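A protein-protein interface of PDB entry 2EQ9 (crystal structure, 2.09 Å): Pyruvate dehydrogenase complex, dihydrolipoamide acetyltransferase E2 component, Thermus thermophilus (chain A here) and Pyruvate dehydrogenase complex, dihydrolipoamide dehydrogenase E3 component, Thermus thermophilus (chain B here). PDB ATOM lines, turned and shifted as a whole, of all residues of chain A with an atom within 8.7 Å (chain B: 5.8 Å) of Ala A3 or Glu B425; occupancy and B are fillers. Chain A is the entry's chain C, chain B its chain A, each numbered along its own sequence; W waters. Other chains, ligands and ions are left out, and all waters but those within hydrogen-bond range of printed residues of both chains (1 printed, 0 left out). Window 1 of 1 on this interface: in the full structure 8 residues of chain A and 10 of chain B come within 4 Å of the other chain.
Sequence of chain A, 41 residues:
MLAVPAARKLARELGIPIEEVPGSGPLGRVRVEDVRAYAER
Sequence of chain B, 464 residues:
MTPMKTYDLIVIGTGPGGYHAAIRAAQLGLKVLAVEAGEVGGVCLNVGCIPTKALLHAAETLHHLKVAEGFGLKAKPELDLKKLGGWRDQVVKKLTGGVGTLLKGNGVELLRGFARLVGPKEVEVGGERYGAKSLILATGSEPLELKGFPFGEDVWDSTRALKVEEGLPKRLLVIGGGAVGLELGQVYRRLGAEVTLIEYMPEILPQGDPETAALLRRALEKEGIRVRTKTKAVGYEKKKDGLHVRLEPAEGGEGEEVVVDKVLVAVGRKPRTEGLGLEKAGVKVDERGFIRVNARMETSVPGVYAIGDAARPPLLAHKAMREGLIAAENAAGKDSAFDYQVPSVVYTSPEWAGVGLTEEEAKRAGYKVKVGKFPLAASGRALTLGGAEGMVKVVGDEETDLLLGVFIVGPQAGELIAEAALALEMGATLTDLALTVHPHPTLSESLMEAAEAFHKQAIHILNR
N of Gln B341 is in hydrogen-bond range of OE1 of Glu B425. O of Leu A2 sits at hydrogen-bond distance from N of Val A30 (2.9 Å). The backbone carbonyl oxygen (O) of Ala A3 lies within hydrogen-bond range of the guanidinium group (NH1) of Arg A8 (2.7 Å). The backbone NH (N) of Val A4 lies within hydrogen-bond range of the backbone carbonyl oxygen (O) of Val A30 (3.3 Å). The backbone NH (N) of Arg A31 sits at hydrogen-bond distance from the side-chain carboxylate (OD2) of Asp A34.
OD2 of Asp B339 lies within salt-bridge range of NE of Arg A8, 2.9 Å away. OE2 of Glu B425 is in salt-bridge range of NH2 of Arg A8. NE of Arg A29 lies within hydrogen-bond range of O of Met B426, 2.8 Å away. O of Gly B427 lies within hydrogen-bond range of NH2 of Arg A29, at 2.8 Å.
Ala A3 touches one residue of chain B. Glu B425 touches four residues of chain A. Of the printed residues of chain B, Val A4 touches Glu B425 (3.7 Å) and Met B426 (3.95 Å). Of the printed residues of chain B, Arg A8 touches Asp B339 (2.9 Å), Tyr B340 (3.4 Å) and Glu B425 (2.9 Å). Printed residues of chain B within 4 Å of Arg A29: Met B426 and Gly B427. Lys A9 touches none of the printed residues of chain B. The nearest printed residue of chain B that does not touch Ala A3 is Met B426 (5.9 Å). The nearest residue of chain A that does not touch Glu B425 is Leu A2 (6.3 Å).
Hydrophobic or aromatic side chains of chain B within 4 Å of the printed part of chain A: Tyr B340 and Met B426. Among the printed residues, 11 pairs touch across the chains. Among the printed residues, Asp or Glu carboxylates within 4 Å of a Lys or Arg side-chain nitrogen of the other chain: Arg A8 with Asp B339 (2.9 Å) and Arg A8 with Glu B425 (2.9 Å).
Among the printed residues, merely in contact across the chains: Arg A8 with Tyr B340 (3.4 Å), Pro A5 with Glu B425 (3.5 Å), Arg A31 with Met B426 (3.6 Å), Val A4 with Glu B425 (3.7 Å), Ala A3 with Glu B425 (3.8 Å), Val A4 with Met B426 (3.95 Å) and Leu A2 with Gly B427 (3.98 Å).
Water W1 lies within hydrogen-bond range of the side-chain carboxylate of Glu B425 (2.6 Å), the backbone carbonyl oxygen of Asp B339 (3.0 Å) and the guanidinium group of Arg A8 (3.4 Å).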
ATOM      1  N   MET A   1      10.664  11.620  20.937  1.00  0.00           N
ATOM      2  CA  MET A   1      10.690  12.235  22.294  1.00  0.00           C
ATOM      3  C   MET A   1       9.474  13.115  22.529  1.00  0.00           C
ATOM      4  O   MET A   1       9.063  13.878  21.653  1.00  0.00           O
ATOM      5  CB  MET A   1      11.946  13.090  22.476  1.00  0.00           C
ATOM      6  CG  MET A   1      11.953  13.885  23.779  1.00  0.00           C
ATOM      7  SD  MET A   1      12.566  15.570  23.560  1.00  0.00           S
ATOM      8  CE  MET A   1      11.050  16.443  23.161  1.00  0.00           C
ATOM      9  N   LEU A   2       8.899  13.006  23.722  1.00  0.00           N
ATOM     10  CA  LEU A   2       7.744  13.813  24.078  1.00  0.00           C
ATOM     11  C   LEU A   2       8.000  14.562  25.384  1.00  0.00           C
ATOM     12  O   LEU A   2       8.143  13.956  26.447  1.00  0.00           O
ATOM     13  CB  LEU A   2       6.481  12.940  24.180  1.00  0.00           C
ATOM     14  CG  LEU A   2       6.442  11.641  24.990  1.00  0.00           C
ATOM     15  CD1 LEU A   2       5.027  11.081  24.948  1.00  0.00           C
ATOM     16  CD2 LEU A   2       7.425  10.624  24.428  1.00  0.00           C
ATOM     17  N   ALA A   3       8.074  15.886  25.282  1.00  0.00           N
ATOM     18  CA  ALA A   3       8.322  16.744  26.433  1.00  0.00           C
ATOM     19  C   ALA A   3       7.313  17.896  26.508  1.00  0.00           C
ATOM     20  O   ALA A   3       7.132  18.648  25.541  1.00  0.00           O
ATOM     21  CB  ALA A   3       9.734  17.296  26.363  1.00  0.00           C
ATOM     22  N   VAL A   4       6.655  18.024  27.658  1.00  0.00           N
ATOM     23  CA  VAL A   4       5.678  19.085  27.852  1.00  0.00           C
ATOM     24  C   VAL A   4       6.420  20.408  27.707  1.00  0.00           C
ATOM     25  O   VAL A   4       7.619  20.477  27.963  1.00  0.00           O
ATOM     26  CB  VAL A   4       5.023  18.999  29.245  1.00  0.00           C
ATOM     27  CG1 VAL A   4       4.507  17.587  29.475  1.00  0.00           C
ATOM     28  CG2 VAL A   4       6.023  19.394  30.333  1.00  0.00           C
ATOM     29  N   PRO A   5       5.723  21.467  27.272  1.00  0.00           N
ATOM     30  CA  PRO A   5       6.340  22.785  27.091  1.00  0.00           C
ATOM     31  C   PRO A   5       7.146  23.279  28.307  1.00  0.00           C
ATOM     32  O   PRO A   5       8.253  23.792  28.157  1.00  0.00           O
ATOM     33  CB  PRO A   5       5.146  23.692  26.791  1.00  0.00           C
ATOM     34  CG  PRO A   5       4.151  22.757  26.154  1.00  0.00           C
ATOM     35  CD  PRO A   5       4.272  21.526  27.017  1.00  0.00           C
ATOM     36  N   ALA A   6       6.592  23.130  29.506  1.00  0.00           N
ATOM     37  CA  ALA A   6       7.287  23.581  30.710  1.00  0.00           C
ATOM     38  C   ALA A   6       8.676  22.949  30.836  1.00  0.00           C
ATOM     39  O   ALA A   6       9.635  23.613  31.231  1.00  0.00           O
ATOM     40  CB  ALA A   6       6.450  23.263  31.954  1.00  0.00           C
ATOM     41  N   ALA A   7       8.778  21.666  30.504  1.00  0.00           N
ATOM     42  CA  ALA A   7      10.057  20.969  30.579  1.00  0.00           C
ATOM     43  C   ALA A   7      11.027  21.448  29.495  1.00  0.00           C
ATOM     44  O   ALA A   7      12.216  21.645  29.764  1.00  0.00           O
ATOM     45  CB  ALA A   7       9.836  19.455  30.467  1.00  0.00           C
ATOM     46  N   ARG A   8      10.524  21.645  28.277  1.00  0.00           N
ATOM     47  CA  ARG A   8      11.372  22.099  27.172  1.00  0.00           C
ATOM     48  C   ARG A   8      11.905  23.494  27.487  1.00  0.00           C
ATOM     49  O   ARG A   8      13.057  23.820  27.191  1.00  0.00           O
ATOM     50  CB  ARG A   8      10.582  22.137  25.851  1.00  0.00           C
ATOM     51  CG  ARG A   8       9.710  20.906  25.624  1.00  0.00           C
ATOM     52  CD  ARG A   8       9.298  20.724  24.172  1.00  0.00           C
ATOM     53  NE  ARG A   8       8.506  21.820  23.615  1.00  0.00           N
ATOM     54  CZ  ARG A   8       7.177  21.847  23.551  1.00  0.00           C
ATOM     55  NH1 ARG A   8       6.460  20.835  24.021  1.00  0.00           N
ATOM     56  NH2 ARG A   8       6.563  22.874  22.968  1.00  0.00           N
ATOM     57  N   LYS A   9      11.049  24.308  28.097  1.00  0.00           N
ATOM     58  CA  LYS A   9      11.403  25.669  28.461  1.00  0.00           C
ATOM     59  C   LYS A   9      12.524  25.660  29.495  1.00  0.00           C
ATOM     60  O   LYS A   9      13.530  26.355  29.342  1.00  0.00           O
ATOM     61  CB  LYS A   9      10.168  26.385  29.014  1.00  0.00           C
ATOM     62  CG  LYS A   9      10.229  27.899  28.910  1.00  0.00           C
ATOM     63  CD  LYS A   9      10.825  28.527  30.152  1.00  0.00           C
ATOM     64  CE  LYS A   9       9.834  28.512  31.308  1.00  0.00           C
ATOM     65  NZ  LYS A   9      10.451  29.078  32.546  1.00  0.00           N
ATOM     66  N   ALA A  11      14.533  23.119  30.225  1.00  0.00           N
ATOM     67  CA  ALA A  11      15.715  22.435  29.713  1.00  0.00           C
ATOM     68  C   ALA A  11      16.636  23.443  29.026  1.00  0.00           C
ATOM     69  O   ALA A  11      17.852  23.429  29.226  1.00  0.00           O
ATOM     70  CB  ALA A  11      15.307  21.343  28.734  1.00  0.00           C
ATOM     71  N   ILE A  18      17.176  18.829  25.661  1.00  0.00           N
ATOM     72  CA  ILE A  18      15.963  18.120  26.055  1.00  0.00           C
ATOM     73  C   ILE A  18      15.896  16.652  25.647  1.00  0.00           C
ATOM     74  O   ILE A  18      15.387  15.821  26.402  1.00  0.00           O
ATOM     75  CB  ILE A  18      14.691  18.844  25.533  1.00  0.00           C
ATOM     76  CG1 ILE A  18      13.441  18.205  26.146  1.00  0.00           C
ATOM     77  CG2 ILE A  18      14.631  18.784  24.009  1.00  0.00           C
ATOM     78  CD1 ILE A  18      13.374  18.310  27.663  1.00  0.00           C
ATOM     79  N   GLU A  19      16.401  16.326  24.463  1.00  0.00           N
ATOM     80  CA  GLU A  19      16.368  14.941  24.004  1.00  0.00           C
ATOM     81  C   GLU A  19      17.274  14.033  24.828  1.00  0.00           C
ATOM     82  O   GLU A  19      17.279  12.817  24.642  1.00  0.00           O
ATOM     83  CB  GLU A  19      16.753  14.851  22.519  1.00  0.00           C
ATOM     84  CG  GLU A  19      17.891  15.765  22.085  1.00  0.00           C
ATOM     85  CD  GLU A  19      17.463  17.217  21.999  1.00  0.00           C
ATOM     86  OE1 GLU A  19      16.400  17.483  21.400  1.00  0.00           O
ATOM     87  OE2 GLU A  19      18.188  18.091  22.521  1.00  0.00           O
ATOM     88  N   VAL A  21      17.213  14.221  28.264  1.00  0.00           N
ATOM     89  CA  VAL A  21      16.564  14.052  29.563  1.00  0.00           C
ATOM     90  C   VAL A  21      15.611  12.857  29.587  1.00  0.00           C
ATOM     91  O   VAL A  21      14.615  12.830  28.864  1.00  0.00           O
ATOM     92  CB  VAL A  21      15.760  15.307  29.959  1.00  0.00           C
ATOM     93  CG1 VAL A  21      15.158  15.121  31.344  1.00  0.00           C
ATOM     94  CG2 VAL A  21      16.654  16.529  29.928  1.00  0.00           C
ATOM     95  N   GLY A  23      12.618  10.435  30.468  1.00  0.00           N
ATOM     96  CA  GLY A  23      11.255  10.690  30.904  1.00  0.00           C
ATOM     97  C   GLY A  23      10.869  10.012  32.204  1.00  0.00           C
ATOM     98  O   GLY A  23      11.733   9.650  33.005  1.00  0.00           O
ATOM     99  N   LEU A  27       5.770   5.765  29.388  1.00  0.00           N
ATOM    100  CA  LEU A  27       6.704   5.668  28.278  1.00  0.00           C
ATOM    101  C   LEU A  27       7.396   6.964  27.845  1.00  0.00           C
ATOM    102  O   LEU A  27       7.132   7.499  26.768  1.00  0.00           O
ATOM    103  CB  LEU A  27       6.031   5.002  27.071  1.00  0.00           C
ATOM    104  CG  LEU A  27       6.901   3.976  26.323  1.00  0.00           C
ATOM    105  CD1 LEU A  27       8.081   4.669  25.645  1.00  0.00           C
ATOM    106  CD2 LEU A  27       7.399   2.912  27.305  1.00  0.00           C
ATOM    107  N   GLY A  28       8.269   7.464  28.717  1.00  0.00           N
ATOM    108  CA  GLY A  28       9.078   8.635  28.418  1.00  0.00           C
ATOM    109  C   GLY A  28       8.639  10.089  28.440  1.00  0.00           C
ATOM    110  O   GLY A  28       9.469  10.953  28.158  1.00  0.00           O
ATOM    111  N   ARG A  29       7.389  10.399  28.760  1.00  0.00           N
ATOM    112  CA  ARG A  29       6.997  11.805  28.766  1.00  0.00           C
ATOM    113  C   ARG A  29       7.876  12.578  29.746  1.00  0.00           C
ATOM    114  O   ARG A  29       7.902  12.282  30.939  1.00  0.00           O
ATOM    115  CB  ARG A  29       5.521  11.965  29.146  1.00  0.00           C
ATOM    116  CG  ARG A  29       5.025  13.403  29.039  1.00  0.00           C
ATOM    117  CD  ARG A  29       3.546  13.557  29.391  1.00  0.00           C
ATOM    118  NE  ARG A  29       2.651  13.027  28.365  1.00  0.00           N
ATOM    119  CZ  ARG A  29       2.167  11.790  28.351  1.00  0.00           C
ATOM    120  NH1 ARG A  29       2.487  10.934  29.313  1.00  0.00           N
ATOM    121  NH2 ARG A  29       1.350  11.409  27.376  1.00  0.00           N
ATOM    122  N   VAL A  30       8.610  13.560  29.234  1.00  0.00           N
ATOM    123  CA  VAL A  30       9.492  14.366  30.072  1.00  0.00           C
ATOM    124  C   VAL A  30       8.739  15.490  30.782  1.00  0.00           C
ATOM    125  O   VAL A  30       8.052  16.294  30.146  1.00  0.00           O
ATOM    126  CB  VAL A  30      10.627  14.976  29.235  1.00  0.00           C
ATOM    127  CG1 VAL A  30      11.608  15.703  30.137  1.00  0.00           C
ATOM    128  CG2 VAL A  30      11.327  13.880  28.436  1.00  0.00           C
ATOM    129  N   ARG A  31       8.875  15.538  32.105  1.00  0.00           N
ATOM    130  CA  ARG A  31       8.224  16.555  32.925  1.00  0.00           C
ATOM    131  C   ARG A  31       9.270  17.487  33.513  1.00  0.00           C
ATOM    132  O   ARG A  31      10.455  17.167  33.518  1.00  0.00           O
ATOM    133  CB  ARG A  31       7.460  15.903  34.076  1.00  0.00           C
ATOM    134  CG  ARG A  31       6.397  14.924  33.652  1.00  0.00           C
ATOM    135  CD  ARG A  31       5.209  15.630  33.035  1.00  0.00           C
ATOM    136  NE  ARG A  31       4.122  14.688  32.796  1.00  0.00           N
ATOM    137  CZ  ARG A  31       2.851  15.036  32.614  1.00  0.00           C
ATOM    138  NH1 ARG A  31       1.934  14.098  32.401  1.00  0.00           N
ATOM    139  NH2 ARG A  31       2.494  16.313  32.651  1.00  0.00           N
ATOM    140  N   VAL A  32       8.822  18.636  34.011  1.00  0.00           N
ATOM    141  CA  VAL A  32       9.718  19.612  34.630  1.00  0.00           C
ATOM    142  C   VAL A  32      10.562  18.941  35.714  1.00  0.00           C
ATOM    143  O   VAL A  32      11.733  19.272  35.896  1.00  0.00           O
ATOM    144  CB  VAL A  32       8.919  20.778  35.267  1.00  0.00           C
ATOM    145  CG1 VAL A  32       9.800  21.561  36.240  1.00  0.00           C
ATOM    146  CG2 VAL A  32       8.411  21.703  34.181  1.00  0.00           C
ATOM    147  N   ASP A  34      11.613  15.798  35.814  1.00  0.00           N
ATOM    148  CA  ASP A  34      12.667  15.030  35.156  1.00  0.00           C
ATOM    149  C   ASP A  34      13.835  15.912  34.715  1.00  0.00           C
ATOM    150  O   ASP A  34      14.997  15.559  34.910  1.00  0.00           O
ATOM    151  CB  ASP A  34      12.108  14.287  33.940  1.00  0.00           C
ATOM    152  CG  ASP A  34      10.944  13.387  34.291  1.00  0.00           C
ATOM    153  OD1 ASP A  34      11.048  12.645  35.292  1.00  0.00           O
ATOM    154  OD2 ASP A  34       9.929  13.414  33.563  1.00  0.00           O
ATOM    155  N   VAL A  35      13.529  17.057  34.117  1.00  0.00           N
ATOM    156  CA  VAL A  35      14.578  17.956  33.660  1.00  0.00           C
ATOM    157  C   VAL A  35      15.446  18.382  34.842  1.00  0.00           C
ATOM    158  O   VAL A  35      16.671  18.424  34.740  1.00  0.00           O
ATOM    159  CB  VAL A  35      13.987  19.206  32.975  1.00  0.00           C
ATOM    160  CG1 VAL A  35      15.106  20.114  32.492  1.00  0.00           C
ATOM    161  CG2 VAL A  35      13.118  18.788  31.803  1.00  0.00           C
ATOM    162  N   ASP B 339       8.989  26.062  19.133  1.00  0.00           N
ATOM    163  CA  ASP B 339       8.886  24.644  18.798  1.00  0.00           C
ATOM    164  C   ASP B 339       7.463  24.188  19.089  1.00  0.00           C
ATOM    165  O   ASP B 339       7.241  23.045  19.474  1.00  0.00           O
ATOM    166  CB  ASP B 339       9.867  23.821  19.645  1.00  0.00           C
ATOM    167  CG  ASP B 339       9.597  23.942  21.144  1.00  0.00           C
ATOM    168  OD1 ASP B 339       8.675  24.701  21.541  1.00  0.00           O
ATOM    169  OD2 ASP B 339      10.312  23.279  21.930  1.00  0.00           O
ATOM    170  N   TYR B 340       6.501  25.084  18.885  1.00  0.00           N
ATOM    171  CA  TYR B 340       5.106  24.794  19.186  1.00  0.00           C
ATOM    172  C   TYR B 340       4.212  24.403  18.017  1.00  0.00           C
ATOM    173  O   TYR B 340       4.519  24.682  16.856  1.00  0.00           O
ATOM    174  CB  TYR B 340       4.476  26.002  19.885  1.00  0.00           C
ATOM    175  CG  TYR B 340       5.297  26.529  21.038  1.00  0.00           C
ATOM    176  CD1 TYR B 340       6.198  27.578  20.863  1.00  0.00           C
ATOM    177  CD2 TYR B 340       5.202  25.948  22.299  1.00  0.00           C
ATOM    178  CE1 TYR B 340       6.990  28.036  21.927  1.00  0.00           C
ATOM    179  CE2 TYR B 340       5.989  26.390  23.361  1.00  0.00           C
ATOM    180  CZ  TYR B 340       6.876  27.426  23.168  1.00  0.00           C
ATOM    181  OH  TYR B 340       7.665  27.827  24.216  1.00  0.00           O
ATOM    182  N   GLN B 341       3.094  23.759  18.355  1.00  0.00           N
ATOM    183  CA  GLN B 341       2.091  23.345  17.384  1.00  0.00           C
ATOM    184  C   GLN B 341       1.292  24.611  17.098  1.00  0.00           C
ATOM    185  O   GLN B 341       0.856  25.291  18.023  1.00  0.00           O
ATOM    186  CB  GLN B 341       1.164  22.295  17.996  1.00  0.00           C
ATOM    187  CG  GLN B 341       1.849  21.004  18.422  1.00  0.00           C
ATOM    188  CD  GLN B 341       2.241  20.132  17.240  1.00  0.00           C
ATOM    189  OE1 GLN B 341       1.511  20.037  16.254  1.00  0.00           O
ATOM    190  NE2 GLN B 341       3.389  19.476  17.344  1.00  0.00           N
ATOM    191  N   ALA B 420      -7.100  20.542  21.381  1.00  0.00           N
ATOM    192  CA  ALA B 420      -6.300  19.648  20.558  1.00  0.00           C
ATOM    193  C   ALA B 420      -4.850  20.086  20.606  1.00  0.00           C
ATOM    194  O   ALA B 420      -3.949  19.259  20.738  1.00  0.00           O
ATOM    195  CB  ALA B 420      -6.800  19.666  19.114  1.00  0.00           C
ATOM    196  N   ALA B 421      -4.625  21.391  20.497  1.00  0.00           N
ATOM    197  CA  ALA B 421      -3.263  21.911  20.534  1.00  0.00           C
ATOM    198  C   ALA B 421      -2.611  21.553  21.865  1.00  0.00           C
ATOM    199  O   ALA B 421      -1.457  21.131  21.895  1.00  0.00           O
ATOM    200  CB  ALA B 421      -3.256  23.428  20.326  1.00  0.00           C
ATOM    201  N   LEU B 422      -3.349  21.724  22.963  1.00  0.00           N
ATOM    202  CA  LEU B 422      -2.813  21.402  24.282  1.00  0.00           C
ATOM    203  C   LEU B 422      -2.505  19.916  24.352  1.00  0.00           C
ATOM    204  O   LEU B 422      -1.503  19.513  24.934  1.00  0.00           O
ATOM    205  CB  LEU B 422      -3.814  21.740  25.394  1.00  0.00           C
ATOM    206  CG  LEU B 422      -3.314  21.299  26.781  1.00  0.00           C
ATOM    207  CD1 LEU B 422      -2.048  22.052  27.111  1.00  0.00           C
ATOM    208  CD2 LEU B 422      -4.373  21.541  27.848  1.00  0.00           C
ATOM    209  N   ALA B 423      -3.392  19.109  23.770  1.00  0.00           N
ATOM    210  CA  ALA B 423      -3.226  17.664  23.752  1.00  0.00           C
ATOM    211  C   ALA B 423      -1.896  17.323  23.083  1.00  0.00           C
ATOM    212  O   ALA B 423      -1.104  16.544  23.608  1.00  0.00           O
ATOM    213  CB  ALA B 423      -4.399  17.009  23.002  1.00  0.00           C
ATOM    214  N   LEU B 424      -1.644  17.928  21.933  1.00  0.00           N
ATOM    215  CA  LEU B 424      -0.404  17.693  21.203  1.00  0.00           C
ATOM    216  C   LEU B 424       0.818  18.137  22.006  1.00  0.00           C
ATOM    217  O   LEU B 424       1.796  17.395  22.122  1.00  0.00           O
ATOM    218  CB  LEU B 424      -0.438  18.439  19.863  1.00  0.00           C
ATOM    219  CG  LEU B 424      -1.479  17.945  18.849  1.00  0.00           C
ATOM    220  CD1 LEU B 424      -1.472  18.847  17.611  1.00  0.00           C
ATOM    221  CD2 LEU B 424      -1.172  16.489  18.470  1.00  0.00           C
ATOM    222  N   GLU B 425       0.764  19.349  22.557  1.00  0.00           N
ATOM    223  CA  GLU B 425       1.876  19.877  23.346  1.00  0.00           C
ATOM    224  C   GLU B 425       2.223  18.976  24.529  1.00  0.00           C
ATOM    225  O   GLU B 425       3.383  18.890  24.923  1.00  0.00           O
ATOM    226  CB  GLU B 425       1.551  21.289  23.871  1.00  0.00           C
ATOM    227  CG  GLU B 425       1.536  22.394  22.809  1.00  0.00           C
ATOM    228  CD  GLU B 425       2.891  22.606  22.148  1.00  0.00           C
ATOM    229  OE1 GLU B 425       2.978  23.419  21.196  1.00  0.00           O
ATOM    230  OE2 GLU B 425       3.872  21.966  22.575  1.00  0.00           O
ATOM    231  N   MET B 426       1.216  18.320  25.094  1.00  0.00           N
ATOM    232  CA  MET B 426       1.405  17.445  26.251  1.00  0.00           C
ATOM    233  C   MET B 426       1.717  15.988  25.889  1.00  0.00           C
ATOM    234  O   MET B 426       1.861  15.155  26.782  1.00  0.00           O
ATOM    235  CB  MET B 426       0.152  17.462  27.148  1.00  0.00           C
ATOM    236  CG  MET B 426      -0.194  18.807  27.775  1.00  0.00           C
ATOM    237  SD  MET B 426       1.060  19.477  28.896  1.00  0.00           S
ATOM    238  CE  MET B 426       0.766  18.514  30.347  1.00  0.00           C
ATOM    239  N   GLY B 427       1.813  15.687  24.594  1.00  0.00           N
ATOM    240  CA  GLY B 427       2.101  14.327  24.156  1.00  0.00           C
ATOM    241  C   GLY B 427       0.974  13.352  24.451  1.00  0.00           C
ATOM    242  O   GLY B 427       1.202  12.169  24.722  1.00  0.00           O
ATOM    243  N   ALA B 428      -0.255  13.847  24.394  1.00  0.00           N
ATOM    244  CA  ALA B 428      -1.422  13.025  24.678  1.00  0.00           C
ATOM    245  C   ALA B 428      -1.630  11.881  23.694  1.00  0.00           C
ATOM    246  O   ALA B 428      -1.230  11.963  22.538  1.00  0.00           O
ATOM    247  CB  ALA B 428      -2.664  13.897  24.699  1.00  0.00           C
HETATM  248  O   HOH W   1       5.097  21.179  20.418  1.00  0.00           O
